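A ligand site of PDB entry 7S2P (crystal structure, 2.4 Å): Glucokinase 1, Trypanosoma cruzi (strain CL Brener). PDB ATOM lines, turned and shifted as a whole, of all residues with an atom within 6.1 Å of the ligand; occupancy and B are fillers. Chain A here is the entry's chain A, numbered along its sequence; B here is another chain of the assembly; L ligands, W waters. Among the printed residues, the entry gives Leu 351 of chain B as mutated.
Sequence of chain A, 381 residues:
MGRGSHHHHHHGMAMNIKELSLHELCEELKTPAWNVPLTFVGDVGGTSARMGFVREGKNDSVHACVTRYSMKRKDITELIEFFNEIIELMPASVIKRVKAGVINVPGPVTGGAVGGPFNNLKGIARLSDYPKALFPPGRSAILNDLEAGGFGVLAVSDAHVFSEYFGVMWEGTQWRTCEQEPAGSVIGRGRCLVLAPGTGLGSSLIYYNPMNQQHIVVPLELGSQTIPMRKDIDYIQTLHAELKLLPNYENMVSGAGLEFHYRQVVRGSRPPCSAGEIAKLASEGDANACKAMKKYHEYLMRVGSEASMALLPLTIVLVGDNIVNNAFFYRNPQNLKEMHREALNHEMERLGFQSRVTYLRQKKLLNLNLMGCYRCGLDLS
Water W1 lies within hydrogen-bond range of O2 of the ligand (2.7 Å), O of Leu 220 (3.0 Å) and N of Ser 203 (3.0 Å).
O of Met 348 of chain B lies within hydrogen-bond range of N of Phe 353 of chain B (3.5 Å). The side-chain carboxylate of Glu 250 sits at hydrogen-bond distance from the backbone NH of Leu 201 (2.7 Å). The side-chain amide nitrogen of Asn 144 is in hydrogen-bond range of the backbone carbonyl oxygen of Gly 107, at 2.7 Å. O of Val 105 is in hydrogen-bond range of N of Asp 145 (3.0 Å). The side-chain carboxylate (OD1) of Asp 145 sits close to the side-chain amide oxygen (OD1) of Asn 144. The backbone carbonyl oxygen of Ala 196 lies within hydrogen-bond range of the backbone NH of Gly 202 (2.9 Å). OD1 of Asn 144 is in hydrogen-bond range of N of Leu 146, at 2.8 Å.
Pro 106 touches the ligand (O to O7, 3.6 Å). Gly 107 touches the ligand. CD of Pro 108 touches C7 of the ligand, at 3.8 Å. Pro 117 touches the ligand (O to C14, 3.3 Å). C of Phe 118 touches C14 of the ligand, at 3.8 Å. Asn 119 touches the ligand. CA of Gly 200 touches O1 of the ligand, 3.5 Å away. Leu 201 touches the ligand. Gly 202 touches the ligand. Met 348 of chain B touches the ligand (CE to C10, 3.6 Å). Leu 351 of chain B touches the ligand. Phe 353 of chain B touches the ligand. Hydrophobic or aromatic side chains within 4 Å of the ligand: Pro 106, Pro 108, Met 348 of chain B, Leu 351 of chain B and Phe 353 of chain B. 16 residues have an atom within 4 Å of the ligand: Pro 106, Gly 107, Pro 108, Pro 117, Phe 118, Asn 119, Asn 144, Asp 145, Gly 200, Leu 201, Gly 202, Glu 221, Glu 250, Met 348 of chain B, Leu 351 of chain B and Phe 353 of chain B.
O2 of the ligand sits at hydrogen-bond distance from OD1 of Asp 145 (2.7 Å). An oxygen (O3) of the ligand is in hydrogen-bond range of the side-chain carboxylate (OE2) of Glu 221, 2.9 Å away. O4 of the ligand sits at hydrogen-bond distance from OE1 of Glu 250, at 3.0 Å. An oxygen (O3) of the ligand lies within hydrogen-bond range of the side-chain amide nitrogen (ND2) of Asn 144.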
ATOM      1  N   VAL A 105     -27.737  22.239   5.624  1.00  0.00           N
ATOM      2  CA  VAL A 105     -28.567  22.838   4.547  1.00  0.00           C
ATOM      3  C   VAL A 105     -27.633  23.292   3.415  1.00  0.00           C
ATOM      4  O   VAL A 105     -26.477  23.668   3.645  1.00  0.00           O
ATOM      5  CB  VAL A 105     -29.375  24.018   5.111  1.00  0.00           C
ATOM      6  CG1 VAL A 105     -30.336  23.508   6.171  1.00  0.00           C
ATOM      7  CG2 VAL A 105     -28.474  25.100   5.714  1.00  0.00           C
ATOM      8  N   PRO A 106     -28.112  23.284   2.159  1.00  0.00           N
ATOM      9  CA  PRO A 106     -27.256  23.533   1.005  1.00  0.00           C
ATOM     10  C   PRO A 106     -27.175  25.021   0.685  1.00  0.00           C
ATOM     11  O   PRO A 106     -27.513  25.412  -0.397  1.00  0.00           O
ATOM     12  CB  PRO A 106     -27.969  22.722  -0.086  1.00  0.00           C
ATOM     13  CG  PRO A 106     -29.415  22.916   0.242  1.00  0.00           C
ATOM     14  CD  PRO A 106     -29.485  22.923   1.758  1.00  0.00           C
ATOM     15  N   GLY A 107     -26.718  25.791   1.656  1.00  0.00           N
ATOM     16  CA  GLY A 107     -26.531  27.242   1.521  1.00  0.00           C
ATOM     17  C   GLY A 107     -25.604  27.771   2.621  1.00  0.00           C
ATOM     18  O   GLY A 107     -25.228  27.034   3.538  1.00  0.00           O
ATOM     19  N   PRO A 108     -25.222  29.050   2.565  1.00  0.00           N
ATOM     20  CA  PRO A 108     -24.337  29.602   3.578  1.00  0.00           C
ATOM     21  C   PRO A 108     -25.115  29.870   4.883  1.00  0.00           C
ATOM     22  O   PRO A 108     -26.287  30.298   4.852  1.00  0.00           O
ATOM     23  CB  PRO A 108     -23.791  30.852   2.911  1.00  0.00           C
ATOM     24  CG  PRO A 108     -24.958  31.299   2.021  1.00  0.00           C
ATOM     25  CD  PRO A 108     -25.605  30.011   1.526  1.00  0.00           C
ATOM     26  N   PRO A 117     -29.641  32.678   1.861  1.00  0.00           N
ATOM     27  CA  PRO A 117     -30.448  32.519   0.646  1.00  0.00           C
ATOM     28  C   PRO A 117     -30.014  31.280  -0.163  1.00  0.00           C
ATOM     29  O   PRO A 117     -28.834  31.068  -0.301  1.00  0.00           O
ATOM     30  CB  PRO A 117     -30.177  33.799  -0.132  1.00  0.00           C
ATOM     31  CG  PRO A 117     -28.873  34.308   0.427  1.00  0.00           C
ATOM     32  CD  PRO A 117     -28.938  33.947   1.896  1.00  0.00           C
ATOM     33  N   PHE A 118     -30.979  30.493  -0.632  1.00  0.00           N
ATOM     34  CA  PHE A 118     -30.658  29.217  -1.321  1.00  0.00           C
ATOM     35  C   PHE A 118     -30.899  29.361  -2.821  1.00  0.00           C
ATOM     36  O   PHE A 118     -31.772  30.152  -3.192  1.00  0.00           O
ATOM     37  CB  PHE A 118     -31.481  28.064  -0.733  1.00  0.00           C
ATOM     38  CG  PHE A 118     -31.247  27.799   0.729  1.00  0.00           C
ATOM     39  CD1 PHE A 118     -30.140  27.081   1.143  1.00  0.00           C
ATOM     40  CD2 PHE A 118     -32.119  28.271   1.686  1.00  0.00           C
ATOM     41  CE1 PHE A 118     -29.922  26.833   2.481  1.00  0.00           C
ATOM     42  CE2 PHE A 118     -31.909  28.003   3.029  1.00  0.00           C
ATOM     43  CZ  PHE A 118     -30.793  27.302   3.429  1.00  0.00           C
ATOM     44  N   ASN A 119     -30.107  28.678  -3.641  1.00  0.00           N
ATOM     45  CA  ASN A 119     -30.316  28.662  -5.120  1.00  0.00           C
ATOM     46  C   ASN A 119     -31.624  27.936  -5.487  1.00  0.00           C
ATOM     47  O   ASN A 119     -32.433  28.522  -6.242  1.00  0.00           O
ATOM     48  CB  ASN A 119     -29.127  28.050  -5.853  1.00  0.00           C
ATOM     49  CG  ASN A 119     -29.104  28.351  -7.342  1.00  0.00           C
ATOM     50  OD1 ASN A 119     -29.853  29.209  -7.853  1.00  0.00           O
ATOM     51  ND2 ASN A 119     -28.274  27.619  -8.059  1.00  0.00           N
ATOM     52  N   ASN A 120     -31.820  26.715  -4.991  1.00  0.00           N
ATOM     53  CA  ASN A 120     -32.956  25.841  -5.405  1.00  0.00           C
ATOM     54  C   ASN A 120     -34.234  26.191  -4.637  1.00  0.00           C
ATOM     55  O   ASN A 120     -35.325  26.213  -5.262  1.00  0.00           O
ATOM     56  CB  ASN A 120     -32.711  24.376  -5.057  1.00  0.00           C
ATOM     57  CG  ASN A 120     -31.381  23.829  -5.568  1.00  0.00           C
ATOM     58  OD1 ASN A 120     -31.042  23.986  -6.737  1.00  0.00           O
ATOM     59  ND2 ASN A 120     -30.660  23.145  -4.692  1.00  0.00           N
ATOM     60  N   ASN A 144     -23.623  24.403   7.115  1.00  0.00           N
ATOM     61  CA  ASN A 144     -23.647  24.309   5.623  1.00  0.00           C
ATOM     62  C   ASN A 144     -23.380  22.849   5.278  1.00  0.00           C
ATOM     63  O   ASN A 144     -22.684  22.165   6.045  1.00  0.00           O
ATOM     64  CB  ASN A 144     -22.679  25.339   5.040  1.00  0.00           C
ATOM     65  CG  ASN A 144     -22.337  25.085   3.594  1.00  0.00           C
ATOM     66  OD1 ASN A 144     -21.466  24.289   3.335  1.00  0.00           O
ATOM     67  ND2 ASN A 144     -23.047  25.701   2.666  1.00  0.00           N
ATOM     68  N   ASP A 145     -23.864  22.369   4.152  1.00  0.00           N
ATOM     69  CA  ASP A 145     -23.721  20.937   3.738  1.00  0.00           C
ATOM     70  C   ASP A 145     -22.231  20.582   3.634  1.00  0.00           C
ATOM     71  O   ASP A 145     -21.875  19.446   4.057  1.00  0.00           O
ATOM     72  CB  ASP A 145     -24.493  20.573   2.463  1.00  0.00           C
ATOM     73  CG  ASP A 145     -24.179  21.436   1.248  1.00  0.00           C
ATOM     74  OD1 ASP A 145     -23.423  22.437   1.370  1.00  0.00           O
ATOM     75  OD2 ASP A 145     -24.697  21.114   0.196  1.00  0.00           O
ATOM     76  N   LEU A 146     -21.365  21.483   3.159  1.00  0.00           N
ATOM     77  CA  LEU A 146     -19.920  21.118   3.062  1.00  0.00           C
ATOM     78  C   LEU A 146     -19.179  21.415   4.374  1.00  0.00           C
ATOM     79  O   LEU A 146     -18.154  20.799   4.609  1.00  0.00           O
ATOM     80  CB  LEU A 146     -19.258  21.758   1.847  1.00  0.00           C
ATOM     81  CG  LEU A 146     -19.201  20.860   0.618  1.00  0.00           C
ATOM     82  CD1 LEU A 146     -18.187  19.736   0.772  1.00  0.00           C
ATOM     83  CD2 LEU A 146     -20.569  20.282   0.261  1.00  0.00           C
ATOM     84  N   ALA A 196     -17.221  19.424  -3.475  1.00  0.00           N
ATOM     85  CA  ALA A 196     -18.375  18.532  -3.729  1.00  0.00           C
ATOM     86  C   ALA A 196     -19.035  19.013  -5.010  1.00  0.00           C
ATOM     87  O   ALA A 196     -19.863  19.882  -4.966  1.00  0.00           O
ATOM     88  CB  ALA A 196     -19.395  18.535  -2.599  1.00  0.00           C
ATOM     89  N   THR A 199     -25.235  18.846  -7.575  1.00  0.00           N
ATOM     90  CA  THR A 199     -26.274  19.832  -7.934  1.00  0.00           C
ATOM     91  C   THR A 199     -25.652  21.230  -7.887  1.00  0.00           C
ATOM     92  O   THR A 199     -25.598  21.895  -8.922  1.00  0.00           O
ATOM     93  CB  THR A 199     -27.421  19.799  -6.917  1.00  0.00           C
ATOM     94  OG1 THR A 199     -27.754  18.446  -6.642  1.00  0.00           O
ATOM     95  CG2 THR A 199     -28.655  20.552  -7.381  1.00  0.00           C
ATOM     96  N   GLY A 200     -25.225  21.631  -6.693  1.00  0.00           N
ATOM     97  CA  GLY A 200     -24.360  22.797  -6.478  1.00  0.00           C
ATOM     98  C   GLY A 200     -22.889  22.407  -6.427  1.00  0.00           C
ATOM     99  O   GLY A 200     -22.616  21.202  -6.321  1.00  0.00           O
ATOM    100  N   LEU A 201     -21.967  23.390  -6.497  1.00  0.00           N
ATOM    101  CA  LEU A 201     -20.528  23.192  -6.223  1.00  0.00           C
ATOM    102  C   LEU A 201     -20.265  23.574  -4.762  1.00  0.00           C
ATOM    103  O   LEU A 201     -20.296  24.720  -4.458  1.00  0.00           O
ATOM    104  CB  LEU A 201     -19.692  23.994  -7.231  1.00  0.00           C
ATOM    105  CG  LEU A 201     -18.172  23.914  -6.981  1.00  0.00           C
ATOM    106  CD1 LEU A 201     -17.713  22.477  -6.854  1.00  0.00           C
ATOM    107  CD2 LEU A 201     -17.345  24.643  -8.042  1.00  0.00           C
ATOM    108  N   GLY A 202     -19.993  22.612  -3.887  1.00  0.00           N
ATOM    109  CA  GLY A 202     -19.760  22.856  -2.452  1.00  0.00           C
ATOM    110  C   GLY A 202     -18.280  22.967  -2.171  1.00  0.00           C
ATOM    111  O   GLY A 202     -17.529  22.490  -2.954  1.00  0.00           O
ATOM    112  N   SER A 203     -17.893  23.689  -1.132  1.00  0.00           N
ATOM    113  CA  SER A 203     -16.466  23.824  -0.781  1.00  0.00           C
ATOM    114  C   SER A 203     -16.382  24.111   0.704  1.00  0.00           C
ATOM    115  O   SER A 203     -17.167  24.955   1.162  1.00  0.00           O
ATOM    116  CB  SER A 203     -15.807  24.895  -1.578  1.00  0.00           C
ATOM    117  OG  SER A 203     -16.451  26.124  -1.406  1.00  0.00           O
ATOM    118  N   LEU A 220     -16.872  27.664   3.045  1.00  0.00           N
ATOM    119  CA  LEU A 220     -16.507  28.540   1.917  1.00  0.00           C
ATOM    120  C   LEU A 220     -17.662  28.579   0.973  1.00  0.00           C
ATOM    121  O   LEU A 220     -18.472  27.617   1.021  1.00  0.00           O
ATOM    122  CB  LEU A 220     -15.249  28.006   1.223  1.00  0.00           C
ATOM    123  CG  LEU A 220     -13.983  27.888   2.080  1.00  0.00           C
ATOM    124  CD1 LEU A 220     -12.874  27.338   1.233  1.00  0.00           C
ATOM    125  CD2 LEU A 220     -13.580  29.206   2.732  1.00  0.00           C
ATOM    126  N   GLU A 221     -17.621  29.554   0.064  1.00  0.00           N
ATOM    127  CA  GLU A 221     -18.423  29.620  -1.165  1.00  0.00           C
ATOM    128  C   GLU A 221     -17.504  29.884  -2.347  1.00  0.00           C
ATOM    129  O   GLU A 221     -17.768  30.829  -3.048  1.00  0.00           O
ATOM    130  CB  GLU A 221     -19.456  30.724  -1.063  1.00  0.00           C
ATOM    131  CG  GLU A 221     -20.424  30.457   0.018  1.00  0.00           C
ATOM    132  CD  GLU A 221     -21.510  29.410  -0.211  1.00  0.00           C
ATOM    133  OE1 GLU A 221     -21.675  29.003  -1.345  1.00  0.00           O
ATOM    134  OE2 GLU A 221     -22.147  28.948   0.807  1.00  0.00           O
ATOM    135  N   SER A 224     -19.210  30.464  -6.050  1.00  0.00           N
ATOM    136  CA  SER A 224     -19.826  31.745  -6.511  1.00  0.00           C
ATOM    137  C   SER A 224     -18.729  32.769  -6.822  1.00  0.00           C
ATOM    138  O   SER A 224     -19.068  33.910  -7.170  1.00  0.00           O
ATOM    139  CB  SER A 224     -20.825  32.216  -5.519  1.00  0.00           C
ATOM    140  OG  SER A 224     -21.690  31.128  -5.157  1.00  0.00           O
ATOM    141  N   GLU A 250     -19.404  27.584 -10.397  1.00  0.00           N
ATOM    142  CA  GLU A 250     -20.581  26.708 -10.268  1.00  0.00           C
ATOM    143  C   GLU A 250     -21.274  26.657 -11.636  1.00  0.00           C
ATOM    144  O   GLU A 250     -21.691  25.555 -12.081  1.00  0.00           O
ATOM    145  CB  GLU A 250     -21.462  27.202  -9.108  1.00  0.00           C
ATOM    146  CG  GLU A 250     -22.745  26.414  -9.011  1.00  0.00           C
ATOM    147  CD  GLU A 250     -23.525  26.559  -7.722  1.00  0.00           C
ATOM    148  OE1 GLU A 250     -23.472  25.609  -6.954  1.00  0.00           O
ATOM    149  OE2 GLU A 250     -24.256  27.570  -7.517  1.00  0.00           O
ATOM    150  N   MET B 309     -17.602  37.046  -1.203  1.00  0.00           N
ATOM    151  CA  MET B 309     -18.400  35.848  -1.536  1.00  0.00           C
ATOM    152  C   MET B 309     -17.652  34.603  -1.035  1.00  0.00           C
ATOM    153  O   MET B 309     -18.269  33.745  -0.359  1.00  0.00           O
ATOM    154  CB  MET B 309     -18.632  35.792  -3.059  1.00  0.00           C
ATOM    155  CG  MET B 309     -19.543  34.735  -3.449  1.00  0.00           C
ATOM    156  SD  MET B 309     -21.162  35.117  -2.782  1.00  0.00           S
ATOM    157  CE  MET B 309     -21.630  33.630  -1.906  1.00  0.00           C
ATOM    158  N   MET B 348     -23.062  38.332  -7.472  1.00  0.00           N
ATOM    159  CA  MET B 348     -23.707  37.847  -6.227  1.00  0.00           C
ATOM    160  C   MET B 348     -24.267  39.008  -5.369  1.00  0.00           C
ATOM    161  O   MET B 348     -24.981  38.754  -4.393  1.00  0.00           O
ATOM    162  CB  MET B 348     -22.696  36.978  -5.465  1.00  0.00           C
ATOM    163  CG  MET B 348     -22.338  35.715  -6.204  1.00  0.00           C
ATOM    164  SD  MET B 348     -23.718  34.644  -6.531  1.00  0.00           S
ATOM    165  CE  MET B 348     -24.242  34.048  -4.941  1.00  0.00           C
ATOM    166  N   ARG B 350     -26.644  40.789  -6.335  1.00  0.00           N
ATOM    167  CA  ARG B 350     -28.096  40.726  -6.596  1.00  0.00           C
ATOM    168  C   ARG B 350     -28.798  40.004  -5.424  1.00  0.00           C
ATOM    169  O   ARG B 350     -30.030  40.131  -5.342  1.00  0.00           O
ATOM    170  CB  ARG B 350     -28.458  40.060  -7.922  1.00  0.00           C
ATOM    171  CG  ARG B 350     -28.293  38.553  -7.899  1.00  0.00           C
ATOM    172  CD  ARG B 350     -28.538  37.919  -9.229  1.00  0.00           C
ATOM    173  NE  ARG B 350     -28.482  36.464  -9.185  1.00  0.00           N
ATOM    174  CZ  ARG B 350     -27.374  35.742  -9.243  1.00  0.00           C
ATOM    175  NH1 ARG B 350     -26.169  36.303  -9.410  1.00  0.00           N
ATOM    176  NH2 ARG B 350     -27.480  34.443  -9.121  1.00  0.00           N
ATOM    177  N   LEU B 351     -28.075  39.300  -4.563  1.00  0.00           N
ATOM    178  CA  LEU B 351     -28.655  38.576  -3.384  1.00  0.00           C
ATOM    179  C   LEU B 351     -28.109  39.147  -2.077  1.00  0.00           C
ATOM    180  O   LEU B 351     -28.319  38.520  -1.086  1.00  0.00           O
ATOM    181  CB  LEU B 351     -28.292  37.099  -3.479  1.00  0.00           C
ATOM    182  CG  LEU B 351     -29.001  36.312  -4.587  1.00  0.00           C
ATOM    183  CD1 LEU B 351     -28.086  35.252  -5.161  1.00  0.00           C
ATOM    184  CD2 LEU B 351     -30.297  35.721  -4.066  1.00  0.00           C
ATOM    185  N   PHE B 353     -24.786  39.640  -1.049  1.00  0.00           N
ATOM    186  CA  PHE B 353     -23.558  39.087  -0.404  1.00  0.00           C
ATOM    187  C   PHE B 353     -22.521  40.179  -0.164  1.00  0.00           C
ATOM    188  O   PHE B 353     -21.909  40.145   0.913  1.00  0.00           O
ATOM    189  CB  PHE B 353     -22.957  37.883  -1.116  1.00  0.00           C
ATOM    190  CG  PHE B 353     -23.795  36.670  -0.871  1.00  0.00           C
ATOM    191  CD1 PHE B 353     -23.716  35.978   0.318  1.00  0.00           C
ATOM    192  CD2 PHE B 353     -24.697  36.240  -1.828  1.00  0.00           C
ATOM    193  CE1 PHE B 353     -24.518  34.875   0.546  1.00  0.00           C
ATOM    194  CE2 PHE B 353     -25.477  35.126  -1.604  1.00  0.00           C
ATOM    195  CZ  PHE B 353     -25.399  34.467  -0.404  1.00  0.00           C
HETATM  196  C1  LIG L   1     -23.462  26.082  -1.247  1.00  0.00           C
HETATM  197  C2  LIG L   1     -24.465  26.633  -2.239  1.00  0.00           C
HETATM  198  C3  LIG L   1     -24.117  26.101  -3.621  1.00  0.00           C
HETATM  199  O1  LIG L   1     -24.312  24.697  -3.554  1.00  0.00           O
HETATM  200  C4  LIG L   1     -23.393  24.081  -2.639  1.00  0.00           C
HETATM  201  C5  LIG L   1     -23.560  24.621  -1.223  1.00  0.00           C
HETATM  202  N1  LIG L   1     -24.300  28.066  -2.236  1.00  0.00           N
HETATM  203  O2  LIG L   1     -22.436  24.135  -0.433  1.00  0.00           O
HETATM  204  O3  LIG L   1     -23.721  26.620   0.029  1.00  0.00           O
HETATM  205  C6  LIG L   1     -23.584  22.571  -2.634  1.00  0.00           C
HETATM  206  O4  LIG L   1     -24.971  26.653  -4.561  1.00  0.00           O
HETATM  207  O5  LIG L   1     -24.978  22.323  -2.261  1.00  0.00           O
HETATM  208  C7  LIG L   1     -25.356  28.864  -2.077  1.00  0.00           C
HETATM  209  O6  LIG L   1     -25.007  30.118  -2.488  1.00  0.00           O
HETATM  210  O7  LIG L   1     -26.487  28.444  -2.068  1.00  0.00           O
HETATM  211  C8  LIG L   1     -26.007  31.123  -2.257  1.00  0.00           C
HETATM  212  C9  LIG L   1     -26.783  31.307  -3.529  1.00  0.00           C
HETATM  213  C10 LIG L   1     -26.194  31.036  -4.776  1.00  0.00           C
HETATM  214  C11 LIG L   1     -26.923  31.211  -5.933  1.00  0.00           C
HETATM  215  C12 LIG L   1     -28.218  31.659  -5.860  1.00  0.00           C
HETATM  216  C13 LIG L   1     -28.796  31.928  -4.642  1.00  0.00           C
HETATM  217  C14 LIG L   1     -28.089  31.765  -3.472  1.00  0.00           C
HETATM  218  O   HOH W   1     -20.142  25.574  -0.309  1.00  0.00           O
